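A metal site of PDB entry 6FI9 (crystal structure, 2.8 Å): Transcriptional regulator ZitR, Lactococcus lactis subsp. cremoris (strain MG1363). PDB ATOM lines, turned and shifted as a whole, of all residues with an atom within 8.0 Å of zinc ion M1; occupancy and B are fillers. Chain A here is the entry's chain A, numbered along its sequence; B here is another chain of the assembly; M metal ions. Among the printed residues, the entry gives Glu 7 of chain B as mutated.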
ATOM      1  N   GLU A  22      10.821  15.254  -8.481  1.00  0.00           N
ATOM      2  CA  GLU A  22      10.032  16.417  -8.879  1.00  0.00           C
ATOM      3  C   GLU A  22       9.279  17.025  -7.701  1.00  0.00           C
ATOM      4  O   GLU A  22       8.958  16.319  -6.736  1.00  0.00           O
ATOM      5  CB  GLU A  22       9.042  16.063 -10.013  1.00  0.00           C
ATOM      6  CG  GLU A  22       8.045  14.962  -9.682  1.00  0.00           C
ATOM      7  CD  GLU A  22       7.208  14.518 -10.865  1.00  0.00           C
ATOM      8  OE1 GLU A  22       6.562  15.379 -11.504  1.00  0.00           O
ATOM      9  OE2 GLU A  22       7.198  13.302 -11.166  1.00  0.00           O
ATOM     10  N   ILE A  23       9.003  18.329  -7.769  1.00  0.00           N
ATOM     11  CA  ILE A  23       8.271  19.036  -6.737  1.00  0.00           C
ATOM     12  C   ILE A  23       6.775  19.089  -7.084  1.00  0.00           C
ATOM     13  O   ILE A  23       6.381  19.636  -8.114  1.00  0.00           O
ATOM     14  CB  ILE A  23       8.885  20.442  -6.415  1.00  0.00           C
ATOM     15  CG1 ILE A  23      10.220  20.291  -5.680  1.00  0.00           C
ATOM     16  CG2 ILE A  23       7.911  21.304  -5.604  1.00  0.00           C
ATOM     17  CD1 ILE A  23      11.061  21.508  -5.726  1.00  0.00           C
ATOM     18  N   LEU A  24       5.954  18.495  -6.204  1.00  0.00           N
ATOM     19  CA  LEU A  24       4.502  18.469  -6.327  1.00  0.00           C
ATOM     20  C   LEU A  24       3.918  18.866  -4.991  1.00  0.00           C
ATOM     21  O   LEU A  24       4.118  18.165  -4.002  1.00  0.00           O
ATOM     22  CB  LEU A  24       4.001  17.077  -6.747  1.00  0.00           C
ATOM     23  CG  LEU A  24       4.123  16.731  -8.238  1.00  0.00           C
ATOM     24  CD1 LEU A  24       4.357  15.245  -8.416  1.00  0.00           C
ATOM     25  CD2 LEU A  24       2.905  17.167  -9.013  1.00  0.00           C
ATOM     26  N   THR A  35       5.568   5.569  -7.284  1.00  0.00           N
ATOM     27  CA  THR A  35       6.483   6.679  -6.997  1.00  0.00           C
ATOM     28  C   THR A  35       6.199   7.906  -7.877  1.00  0.00           C
ATOM     29  O   THR A  35       5.339   7.849  -8.760  1.00  0.00           O
ATOM     30  CB  THR A  35       7.961   6.239  -7.072  1.00  0.00           C
ATOM     31  OG1 THR A  35       8.240   5.682  -8.361  1.00  0.00           O
ATOM     32  CG2 THR A  35       8.349   5.261  -5.973  1.00  0.00           C
ATOM     33  N   SER A  36       6.933   9.017  -7.624  1.00  0.00           N
ATOM     34  CA  SER A  36       6.810  10.285  -8.359  1.00  0.00           C
ATOM     35  C   SER A  36       7.010  10.077  -9.865  1.00  0.00           C
ATOM     36  O   SER A  36       6.127  10.421 -10.656  1.00  0.00           O
ATOM     37  CB  SER A  36       7.804  11.318  -7.814  1.00  0.00           C
ATOM     38  OG  SER A  36       7.637  11.556  -6.423  1.00  0.00           O
ATOM     39  N   THR A  37       8.157   9.466 -10.239  1.00  0.00           N
ATOM     40  CA  THR A  37       8.539   9.180 -11.626  1.00  0.00           C
ATOM     41  C   THR A  37       7.586   8.202 -12.304  1.00  0.00           C
ATOM     42  O   THR A  37       7.152   8.462 -13.429  1.00  0.00           O
ATOM     43  CB  THR A  37      10.007   8.728 -11.712  1.00  0.00           C
ATOM     44  OG1 THR A  37      10.196   7.589 -10.867  1.00  0.00           O
ATOM     45  CG2 THR A  37      10.997   9.827 -11.342  1.00  0.00           C
ATOM     46  N   GLN A  38       7.255   7.090 -11.604  1.00  0.00           N
ATOM     47  CA  GLN A  38       6.356   6.036 -12.089  1.00  0.00           C
ATOM     48  C   GLN A  38       5.003   6.573 -12.562  1.00  0.00           C
ATOM     49  O   GLN A  38       4.530   6.183 -13.639  1.00  0.00           O
ATOM     50  CB  GLN A  38       6.166   4.941 -11.030  1.00  0.00           C
ATOM     51  CG  GLN A  38       7.275   3.901 -11.031  1.00  0.00           C
ATOM     52  CD  GLN A  38       7.068   2.880  -9.935  1.00  0.00           C
ATOM     53  OE1 GLN A  38       7.222   3.172  -8.745  1.00  0.00           O
ATOM     54  NE2 GLN A  38       6.721   1.664 -10.321  1.00  0.00           N
ATOM     55  N   GLU A  39       4.387   7.477 -11.764  1.00  0.00           N
ATOM     56  CA  GLU A  39       3.103   8.089 -12.105  1.00  0.00           C
ATOM     57  C   GLU A  39       3.243   9.055 -13.271  1.00  0.00           C
ATOM     58  O   GLU A  39       2.362   9.115 -14.129  1.00  0.00           O
ATOM     59  CB  GLU A  39       2.484   8.772 -10.884  1.00  0.00           C
ATOM     60  CG  GLU A  39       1.659   7.818 -10.034  1.00  0.00           C
ATOM     61  CD  GLU A  39       0.902   8.428  -8.872  1.00  0.00           C
ATOM     62  OE1 GLU A  39       0.263   9.486  -9.059  1.00  0.00           O
ATOM     63  OE2 GLU A  39       0.935   7.829  -7.763  1.00  0.00           O
ATOM     64  N   HIS A  40       4.379   9.763 -13.321  1.00  0.00           N
ATOM     65  CA  HIS A  40       4.681  10.718 -14.391  1.00  0.00           C
ATOM     66  C   HIS A  40       4.892  10.018 -15.739  1.00  0.00           C
ATOM     67  O   HIS A  40       4.504  10.571 -16.763  1.00  0.00           O
ATOM     68  CB  HIS A  40       5.858  11.627 -14.024  1.00  0.00           C
ATOM     69  CG  HIS A  40       6.072  12.740 -15.003  1.00  0.00           C
ATOM     70  ND1 HIS A  40       5.179  13.794 -15.085  1.00  0.00           N
ATOM     71  CD2 HIS A  40       7.038  12.908 -15.932  1.00  0.00           C
ATOM     72  CE1 HIS A  40       5.641  14.567 -16.058  1.00  0.00           C
ATOM     73  NE2 HIS A  40       6.759  14.078 -16.594  1.00  0.00           N
ATOM     74  N   ILE A  41       5.474   8.790 -15.728  1.00  0.00           N
ATOM     75  CA  ILE A  41       5.683   8.000 -16.939  1.00  0.00           C
ATOM     76  C   ILE A  41       4.309   7.710 -17.582  1.00  0.00           C
ATOM     77  O   ILE A  41       4.154   7.843 -18.792  1.00  0.00           O
ATOM     78  CB  ILE A  41       6.536   6.727 -16.663  1.00  0.00           C
ATOM     79  CG1 ILE A  41       7.986   7.107 -16.308  1.00  0.00           C
ATOM     80  CG2 ILE A  41       6.524   5.758 -17.846  1.00  0.00           C
ATOM     81  CD1 ILE A  41       8.738   6.116 -15.392  1.00  0.00           C
ATOM     82  N   MET A  43       1.579   9.536 -17.229  1.00  0.00           N
ATOM     83  CA  MET A  43       1.062  10.835 -17.654  1.00  0.00           C
ATOM     84  C   MET A  43       1.495  11.192 -19.091  1.00  0.00           C
ATOM     85  O   MET A  43       0.637  11.545 -19.898  1.00  0.00           O
ATOM     86  CB  MET A  43       1.484  11.918 -16.646  1.00  0.00           C
ATOM     87  CG  MET A  43       0.886  13.271 -16.904  1.00  0.00           C
ATOM     88  SD  MET A  43       1.647  14.518 -15.855  1.00  0.00           S
ATOM     89  CE  MET A  43       1.326  15.959 -16.836  1.00  0.00           C
ATOM     90  N   ILE A  44       2.810  11.074 -19.399  1.00  0.00           N
ATOM     91  CA  ILE A  44       3.379  11.368 -20.730  1.00  0.00           C
ATOM     92  C   ILE A  44       2.980  10.319 -21.779  1.00  0.00           C
ATOM     93  O   ILE A  44       2.892  10.648 -22.953  1.00  0.00           O
ATOM     94  CB  ILE A  44       4.924  11.625 -20.720  1.00  0.00           C
ATOM     95  CG1 ILE A  44       5.711  10.440 -20.104  1.00  0.00           C
ATOM     96  CG2 ILE A  44       5.254  12.951 -20.042  1.00  0.00           C
ATOM     97  CD1 ILE A  44       7.061  10.189 -20.746  1.00  0.00           C
ATOM     98  N   LEU A  59      11.638  12.692 -18.973  1.00  0.00           N
ATOM     99  CA  LEU A  59      11.852  12.657 -17.524  1.00  0.00           C
ATOM    100  C   LEU A  59      13.215  13.166 -17.081  1.00  0.00           C
ATOM    101  O   LEU A  59      13.392  13.472 -15.895  1.00  0.00           O
ATOM    102  CB  LEU A  59      11.617  11.239 -16.986  1.00  0.00           C
ATOM    103  CG  LEU A  59      10.205  10.915 -16.532  1.00  0.00           C
ATOM    104  CD1 LEU A  59       9.367  10.372 -17.675  1.00  0.00           C
ATOM    105  CD2 LEU A  59      10.243   9.913 -15.395  1.00  0.00           C
ATOM    106  N   HIS A 106      -2.254  12.561 -11.972  1.00  0.00           N
ATOM    107  CA  HIS A 106      -0.932  13.195 -11.980  1.00  0.00           C
ATOM    108  C   HIS A 106      -0.961  14.505 -12.758  1.00  0.00           C
ATOM    109  O   HIS A 106      -0.372  15.482 -12.316  1.00  0.00           O
ATOM    110  CB  HIS A 106       0.127  12.249 -12.529  1.00  0.00           C
ATOM    111  CG  HIS A 106       1.501  12.542 -12.010  1.00  0.00           C
ATOM    112  ND1 HIS A 106       1.865  12.210 -10.726  1.00  0.00           N
ATOM    113  CD2 HIS A 106       2.548  13.133 -12.633  1.00  0.00           C
ATOM    114  CE1 HIS A 106       3.127  12.604 -10.605  1.00  0.00           C
ATOM    115  NE2 HIS A 106       3.574  13.161 -11.722  1.00  0.00           N
ATOM    116  N   ALA A 107      -1.687  14.533 -13.890  1.00  0.00           N
ATOM    117  CA  ALA A 107      -1.855  15.720 -14.721  1.00  0.00           C
ATOM    118  C   ALA A 107      -2.618  16.812 -13.952  1.00  0.00           C
ATOM    119  O   ALA A 107      -2.350  17.994 -14.118  1.00  0.00           O
ATOM    120  CB  ALA A 107      -2.593  15.353 -15.991  1.00  0.00           C
ATOM    121  N   HIS A 109      -2.561  16.858 -10.529  1.00  0.00           N
ATOM    122  CA  HIS A 109      -1.625  17.130  -9.431  1.00  0.00           C
ATOM    123  C   HIS A 109      -0.542  18.126  -9.877  1.00  0.00           C
ATOM    124  O   HIS A 109      -0.033  18.877  -9.044  1.00  0.00           O
ATOM    125  CB  HIS A 109      -1.005  15.820  -8.910  1.00  0.00           C
ATOM    126  CG  HIS A 109      -0.331  15.913  -7.573  1.00  0.00           C
ATOM    127  ND1 HIS A 109       0.485  14.893  -7.114  1.00  0.00           N
ATOM    128  CD2 HIS A 109      -0.384  16.884  -6.632  1.00  0.00           C
ATOM    129  CE1 HIS A 109       0.907  15.280  -5.919  1.00  0.00           C
ATOM    130  NE2 HIS A 109       0.411  16.477  -5.589  1.00  0.00           N
ATOM    131  N   HIS A 110      -0.196  18.141 -11.169  1.00  0.00           N
ATOM    132  CA  HIS A 110       0.754  19.082 -11.750  1.00  0.00           C
ATOM    133  C   HIS A 110       0.126  20.459 -11.921  1.00  0.00           C
ATOM    134  O   HIS A 110       0.778  21.465 -11.637  1.00  0.00           O
ATOM    135  CB  HIS A 110       1.287  18.565 -13.097  1.00  0.00           C
ATOM    136  CG  HIS A 110       2.613  17.883 -12.977  1.00  0.00           C
ATOM    137  ND1 HIS A 110       3.772  18.604 -12.696  1.00  0.00           N
ATOM    138  CD2 HIS A 110       2.934  16.577 -13.102  1.00  0.00           C
ATOM    139  CE1 HIS A 110       4.744  17.708 -12.668  1.00  0.00           C
ATOM    140  NE2 HIS A 110       4.287  16.469 -12.899  1.00  0.00           N
ATOM    141  N   GLU B   7       7.732  26.980 -11.681  1.00  0.00           N
ATOM    142  CA  GLU B   7       7.848  25.537 -11.924  1.00  0.00           C
ATOM    143  C   GLU B   7       9.217  25.219 -12.543  1.00  0.00           C
ATOM    144  O   GLU B   7       9.829  24.228 -12.163  1.00  0.00           O
ATOM    145  CB  GLU B   7       6.710  25.046 -12.844  1.00  0.00           C
ATOM    146  CG  GLU B   7       6.607  23.518 -12.906  1.00  0.00           C
ATOM    147  CD  GLU B   7       5.545  22.921 -13.826  1.00  0.00           C
ATOM    148  OE1 GLU B   7       5.566  23.227 -15.037  1.00  0.00           O
ATOM    149  OE2 GLU B   7       4.723  22.120 -13.324  1.00  0.00           O
HETATM  150 ZN    ZN M   1       4.941  14.682 -12.430  1.00  0.00          ZN
HETATM  151 ZN    ZN M   2      -0.756  11.510  -8.466  1.00  0.00          ZN
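The nearest printed residue that does not touch zinc ion M1 is Leu 24 (4.1 Å).
SD of Met 43 sits at hydrogen-bond distance from ND1 of His 40 (3.7 Å).
Zinc ion M1 is bound by NE2 of His 110, OE1 of Glu 22 and NE2 of His 106.
Zinc ion M1 has three donor atoms within binding distance.
Slightly farther from zinc ion M1 lies a ring nitrogen (ND1) of His 40 (2.8 Å).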
